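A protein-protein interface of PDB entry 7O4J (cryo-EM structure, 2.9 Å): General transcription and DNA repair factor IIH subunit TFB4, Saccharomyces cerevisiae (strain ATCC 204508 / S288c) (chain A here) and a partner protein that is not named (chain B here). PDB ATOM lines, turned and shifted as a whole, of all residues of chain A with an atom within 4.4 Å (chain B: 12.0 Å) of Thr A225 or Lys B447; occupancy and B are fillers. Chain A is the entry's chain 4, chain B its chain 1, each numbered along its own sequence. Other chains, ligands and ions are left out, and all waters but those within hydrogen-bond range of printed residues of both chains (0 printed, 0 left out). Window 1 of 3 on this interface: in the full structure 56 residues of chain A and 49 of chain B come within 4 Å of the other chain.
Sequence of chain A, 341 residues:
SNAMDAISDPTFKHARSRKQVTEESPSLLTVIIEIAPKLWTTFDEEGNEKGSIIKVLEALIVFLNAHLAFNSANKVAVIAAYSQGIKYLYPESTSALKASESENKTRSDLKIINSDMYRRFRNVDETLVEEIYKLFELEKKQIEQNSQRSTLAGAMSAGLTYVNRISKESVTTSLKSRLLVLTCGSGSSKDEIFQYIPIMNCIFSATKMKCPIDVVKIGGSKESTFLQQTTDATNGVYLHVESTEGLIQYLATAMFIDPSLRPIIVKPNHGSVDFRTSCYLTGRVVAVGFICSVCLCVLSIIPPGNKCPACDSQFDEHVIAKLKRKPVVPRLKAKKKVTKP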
ATOM      1  N   GLU A 192     -26.074 -14.365  -6.274  1.00  0.00           N
ATOM      2  CA  GLU A 192     -26.897 -15.000  -7.293  1.00  0.00           C
ATOM      3  C   GLU A 192     -27.960 -15.922  -6.709  1.00  0.00           C
ATOM      4  O   GLU A 192     -28.747 -16.491  -7.471  1.00  0.00           O
ATOM      5  CB  GLU A 192     -26.016 -15.783  -8.277  1.00  0.00           C
ATOM      6  CG  GLU A 192     -25.335 -17.024  -7.702  1.00  0.00           C
ATOM      7  CD  GLU A 192     -24.092 -16.697  -6.897  1.00  0.00           C
ATOM      8  OE1 GLU A 192     -23.816 -15.497  -6.689  1.00  0.00           O
ATOM      9  OE2 GLU A 192     -23.392 -17.640  -6.472  1.00  0.00           O
ATOM     10  N   ILE A 193     -28.013 -16.071  -5.384  1.00  0.00           N
ATOM     11  CA  ILE A 193     -28.958 -17.004  -4.778  1.00  0.00           C
ATOM     12  C   ILE A 193     -30.389 -16.635  -5.138  1.00  0.00           C
ATOM     13  O   ILE A 193     -31.209 -17.515  -5.434  1.00  0.00           O
ATOM     14  CB  ILE A 193     -28.759 -17.052  -3.250  1.00  0.00           C
ATOM     15  CG1 ILE A 193     -27.326 -17.470  -2.902  1.00  0.00           C
ATOM     16  CG2 ILE A 193     -29.762 -18.002  -2.610  1.00  0.00           C
ATOM     17  CD1 ILE A 193     -26.942 -18.854  -3.395  1.00  0.00           C
ATOM     18  N   GLU A 223     -17.722 -20.893 -15.563  1.00  0.00           N
ATOM     19  CA  GLU A 223     -19.017 -21.545 -15.429  1.00  0.00           C
ATOM     20  C   GLU A 223     -19.990 -20.663 -14.661  1.00  0.00           C
ATOM     21  O   GLU A 223     -19.611 -19.996 -13.693  1.00  0.00           O
ATOM     22  CB  GLU A 223     -18.886 -22.906 -14.722  1.00  0.00           C
ATOM     23  CG  GLU A 223     -18.384 -22.843 -13.280  1.00  0.00           C
ATOM     24  CD  GLU A 223     -16.873 -22.819 -13.186  1.00  0.00           C
ATOM     25  OE1 GLU A 223     -16.230 -22.266 -14.100  1.00  0.00           O
ATOM     26  OE2 GLU A 223     -16.329 -23.356 -12.198  1.00  0.00           O
ATOM     27  N   SER A 224     -21.244 -20.662 -15.108  1.00  0.00           N
ATOM     28  CA  SER A 224     -22.365 -20.093 -14.368  1.00  0.00           C
ATOM     29  C   SER A 224     -23.275 -21.250 -13.982  1.00  0.00           C
ATOM     30  O   SER A 224     -23.930 -21.845 -14.845  1.00  0.00           O
ATOM     31  CB  SER A 224     -23.112 -19.053 -15.200  1.00  0.00           C
ATOM     32  OG  SER A 224     -22.330 -17.885 -15.378  1.00  0.00           O
ATOM     33  N   THR A 225     -23.322 -21.566 -12.686  1.00  0.00           N
ATOM     34  CA  THR A 225     -23.973 -22.798 -12.254  1.00  0.00           C
ATOM     35  C   THR A 225     -25.454 -22.818 -12.609  1.00  0.00           C
ATOM     36  O   THR A 225     -25.995 -23.881 -12.932  1.00  0.00           O
ATOM     37  CB  THR A 225     -23.796 -22.987 -10.748  1.00  0.00           C
ATOM     38  OG1 THR A 225     -22.401 -22.977 -10.423  1.00  0.00           O
ATOM     39  CG2 THR A 225     -24.412 -24.307 -10.304  1.00  0.00           C
ATOM     40  N   PHE A 226     -26.127 -21.670 -12.557  1.00  0.00           N
ATOM     41  CA  PHE A 226     -27.565 -21.634 -12.799  1.00  0.00           C
ATOM     42  C   PHE A 226     -27.907 -21.621 -14.284  1.00  0.00           C
ATOM     43  O   PHE A 226     -28.818 -22.339 -14.710  1.00  0.00           O
ATOM     44  CB  PHE A 226     -28.181 -20.411 -12.114  1.00  0.00           C
ATOM     45  CG  PHE A 226     -28.094 -20.446 -10.610  1.00  0.00           C
ATOM     46  CD1 PHE A 226     -27.841 -21.630  -9.934  1.00  0.00           C
ATOM     47  CD2 PHE A 226     -28.268 -19.288  -9.872  1.00  0.00           C
ATOM     48  CE1 PHE A 226     -27.765 -21.656  -8.556  1.00  0.00           C
ATOM     49  CE2 PHE A 226     -28.191 -19.312  -8.494  1.00  0.00           C
ATOM     50  CZ  PHE A 226     -27.939 -20.496  -7.837  1.00  0.00           C
ATOM     51  N   LEU A 227     -27.200 -20.822 -15.085  1.00  0.00           N
ATOM     52  CA  LEU A 227     -27.492 -20.788 -16.513  1.00  0.00           C
ATOM     53  C   LEU A 227     -27.014 -22.052 -17.216  1.00  0.00           C
ATOM     54  O   LEU A 227     -27.633 -22.484 -18.193  1.00  0.00           O
ATOM     55  CB  LEU A 227     -26.868 -19.547 -17.150  1.00  0.00           C
ATOM     56  CG  LEU A 227     -27.484 -18.214 -16.716  1.00  0.00           C
ATOM     57  CD1 LEU A 227     -26.694 -17.044 -17.275  1.00  0.00           C
ATOM     58  CD2 LEU A 227     -28.941 -18.128 -17.147  1.00  0.00           C
ATOM     59  N   GLN A 228     -25.923 -22.660 -16.740  1.00  0.00           N
ATOM     60  CA  GLN A 228     -25.490 -23.930 -17.313  1.00  0.00           C
ATOM     61  C   GLN A 228     -26.559 -25.000 -17.135  1.00  0.00           C
ATOM     62  O   GLN A 228     -26.843 -25.767 -18.063  1.00  0.00           O
ATOM     63  CB  GLN A 228     -24.179 -24.384 -16.672  1.00  0.00           C
ATOM     64  CG  GLN A 228     -22.942 -23.665 -17.174  1.00  0.00           C
ATOM     65  CD  GLN A 228     -21.667 -24.384 -16.780  1.00  0.00           C
ATOM     66  OE1 GLN A 228     -21.707 -25.448 -16.165  1.00  0.00           O
ATOM     67  NE2 GLN A 228     -20.527 -23.806 -17.136  1.00  0.00           N
ATOM     68  N   GLN A 229     -27.160 -25.070 -15.945  1.00  0.00           N
ATOM     69  CA  GLN A 229     -28.264 -25.999 -15.730  1.00  0.00           C
ATOM     70  C   GLN A 229     -29.446 -25.657 -16.626  1.00  0.00           C
ATOM     71  O   GLN A 229     -30.165 -26.552 -17.083  1.00  0.00           O
ATOM     72  CB  GLN A 229     -28.684 -25.980 -14.261  1.00  0.00           C
ATOM     73  CG  GLN A 229     -27.659 -26.582 -13.317  1.00  0.00           C
ATOM     74  CD  GLN A 229     -28.152 -26.635 -11.885  1.00  0.00           C
ATOM     75  OE1 GLN A 229     -29.349 -26.764 -11.633  1.00  0.00           O
ATOM     76  NE2 GLN A 229     -27.226 -26.534 -10.938  1.00  0.00           N
ATOM     77  N   SER A 278     -26.678 -25.270  -3.391  1.00  0.00           N
ATOM     78  CA  SER A 278     -25.869 -24.875  -2.248  1.00  0.00           C
ATOM     79  C   SER A 278     -26.693 -24.936  -0.969  1.00  0.00           C
ATOM     80  O   SER A 278     -27.915 -24.769  -0.993  1.00  0.00           O
ATOM     81  CB  SER A 278     -25.313 -23.464  -2.442  1.00  0.00           C
ATOM     82  OG  SER A 278     -26.312 -22.589  -2.934  1.00  0.00           O
ATOM     83  N   GLY A 283     -23.519 -22.257   2.477  1.00  0.00           N
ATOM     84  CA  GLY A 283     -23.166 -21.823   1.141  1.00  0.00           C
ATOM     85  C   GLY A 283     -22.171 -22.703   0.423  1.00  0.00           C
ATOM     86  O   GLY A 283     -21.329 -22.187  -0.314  1.00  0.00           O
ATOM     87  N   ASN B 443     -33.167 -15.984   2.885  1.00  0.00           N
ATOM     88  CA  ASN B 443     -31.851 -15.398   3.106  1.00  0.00           C
ATOM     89  C   ASN B 443     -30.829 -16.506   3.321  1.00  0.00           C
ATOM     90  O   ASN B 443     -31.016 -17.372   4.181  1.00  0.00           O
ATOM     91  CB  ASN B 443     -31.877 -14.439   4.299  1.00  0.00           C
ATOM     92  CG  ASN B 443     -32.164 -15.142   5.611  1.00  0.00           C
ATOM     93  OD1 ASN B 443     -31.296 -15.804   6.179  1.00  0.00           O
ATOM     94  ND2 ASN B 443     -33.391 -14.999   6.103  1.00  0.00           N
ATOM     95  N   ALA B 444     -29.754 -16.498   2.538  1.00  0.00           N
ATOM     96  CA  ALA B 444     -28.735 -17.532   2.646  1.00  0.00           C
ATOM     97  C   ALA B 444     -27.410 -16.978   2.146  1.00  0.00           C
ATOM     98  O   ALA B 444     -27.375 -16.026   1.362  1.00  0.00           O
ATOM     99  CB  ALA B 444     -29.119 -18.785   1.854  1.00  0.00           C
ATOM    100  N   HIS B 445     -26.323 -17.585   2.614  1.00  0.00           N
ATOM    101  CA  HIS B 445     -24.994 -17.178   2.186  1.00  0.00           C
ATOM    102  C   HIS B 445     -24.757 -17.566   0.731  1.00  0.00           C
ATOM    103  O   HIS B 445     -25.334 -18.528   0.217  1.00  0.00           O
ATOM    104  CB  HIS B 445     -23.926 -17.820   3.073  1.00  0.00           C
ATOM    105  CG  HIS B 445     -23.584 -17.017   4.290  1.00  0.00           C
ATOM    106  ND1 HIS B 445     -22.610 -17.404   5.184  1.00  0.00           N
ATOM    107  CD2 HIS B 445     -24.086 -15.852   4.763  1.00  0.00           C
ATOM    108  CE1 HIS B 445     -22.525 -16.512   6.155  1.00  0.00           C
ATOM    109  NE2 HIS B 445     -23.411 -15.559   5.922  1.00  0.00           N
ATOM    110  N   GLU B 446     -23.896 -16.801   0.068  1.00  0.00           N
ATOM    111  CA  GLU B 446     -23.540 -17.103  -1.309  1.00  0.00           C
ATOM    112  C   GLU B 446     -22.708 -18.380  -1.375  1.00  0.00           C
ATOM    113  O   GLU B 446     -22.144 -18.842  -0.379  1.00  0.00           O
ATOM    114  CB  GLU B 446     -22.769 -15.940  -1.931  1.00  0.00           C
ATOM    115  CG  GLU B 446     -21.408 -15.678  -1.300  1.00  0.00           C
ATOM    116  CD  GLU B 446     -20.707 -14.475  -1.900  1.00  0.00           C
ATOM    117  OE1 GLU B 446     -21.293 -13.830  -2.795  1.00  0.00           O
ATOM    118  OE2 GLU B 446     -19.571 -14.175  -1.479  1.00  0.00           O
ATOM    119  N   LYS B 447     -22.638 -18.953  -2.573  1.00  0.00           N
ATOM    120  CA  LYS B 447     -21.881 -20.181  -2.763  1.00  0.00           C
ATOM    121  C   LYS B 447     -20.411 -19.954  -2.440  1.00  0.00           C
ATOM    122  O   LYS B 447     -19.813 -18.956  -2.852  1.00  0.00           O
ATOM    123  CB  LYS B 447     -22.033 -20.685  -4.199  1.00  0.00           C
ATOM    124  CG  LYS B 447     -23.456 -20.622  -4.733  1.00  0.00           C
ATOM    125  CD  LYS B 447     -23.791 -21.831  -5.592  1.00  0.00           C
ATOM    126  CE  LYS B 447     -22.813 -21.994  -6.747  1.00  0.00           C
ATOM    127  NZ  LYS B 447     -23.212 -23.104  -7.651  1.00  0.00           N
ATOM    128  N   THR B 448     -19.828 -20.891  -1.696  1.00  0.00           N
ATOM    129  CA  THR B 448     -18.443 -20.812  -1.259  1.00  0.00           C
ATOM    130  C   THR B 448     -17.676 -22.020  -1.776  1.00  0.00           C
ATOM    131  O   THR B 448     -18.176 -23.148  -1.743  1.00  0.00           O
ATOM    132  CB  THR B 448     -18.343 -20.751   0.270  1.00  0.00           C
ATOM    133  OG1 THR B 448     -18.501 -22.067   0.816  1.00  0.00           O
ATOM    134  CG2 THR B 448     -19.412 -19.830   0.844  1.00  0.00           C
ATOM    135  N   THR B 449     -16.460 -21.776  -2.255  1.00  0.00           N
ATOM    136  CA  THR B 449     -15.614 -22.839  -2.783  1.00  0.00           C
ATOM    137  C   THR B 449     -15.333 -23.890  -1.713  1.00  0.00           C
ATOM    138  O   THR B 449     -14.505 -23.680  -0.826  1.00  0.00           O
ATOM    139  CB  THR B 449     -14.277 -22.287  -3.312  1.00  0.00           C
ATOM    140  OG1 THR B 449     -13.561 -21.651  -2.244  1.00  0.00           O
ATOM    141  CG2 THR B 449     -14.516 -21.281  -4.429  1.00  0.00           C
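O of Glu B446 lies close to O of Gly A283, at 3.4 Å. The backbone NH of Thr B448 lies within hydrogen-bond range of the backbone carbonyl oxygen of Gly A283 (2.4 Å). The side-chain hydroxyl (OG1) of Thr A225 is in hydrogen-bond range of the side-chain amino group (NZ) of Lys B447 (2.9 Å).
Among the printed residues, pairs that only touch across the chains: Glu A192 with Lys B447 (3.5 Å), Ile A193 with His B445 (3.8 Å), Ser A278 with Lys B447 (3.7 Å) and Gly A283 with Lys B447 (3.2 Å).
Of chain B, only Lys B447 comes within 4 Å of Glu A192. Of the printed residues of chain B, Ile A193 touches His B445 (3.8 Å). No residue of chain B comes within 4 Å of Glu A223. No residue of chain B comes within 4 Å of Ser A224. Thr A225 touches just one residue of chain B: Lys B447 (2.9 Å). No residue of chain B comes within 4 Å of Gln A228. No residue of chain B comes within 4 Å of Gln A229. Of chain B, only Lys B447 comes within 4 Å of Ser A278. Of chain B, only Glu B446 (3.4 Å), Lys B447 (3.2 Å) and Thr B448 (2.4 Å) come within 4 Å of Gly A283. Of the printed residues of chain A, Glu B446 touches Gly A283 (3.4 Å). Of chain A, only Glu A192 (3.5 Å), Thr A225 (2.9 Å), Ser A278 (3.7 Å) and Gly A283 (3.2 Å) come within 4 Å of Lys B447. Of the printed residues of chain A, Thr B448 touches Gly A283 (2.4 Å). The nearest residue of chain B that does not touch Thr A225 is Thr B448 (9.3 Å). The nearest residue of chain A that does not touch Lys B447 is Ile A193 (4.1 Å). The nearest printed residue of chain B that does not touch Ile A193 is Glu B446 (4.1 Å).
Printed residues of chain B that touch a printed residue of chain A: His B445, Glu B446, Lys B447 and Thr B448. Among the printed residues, no Asp or Glu carboxylate lies within 4 Å of a Lys or Arg side-chain nitrogen of the other chain.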
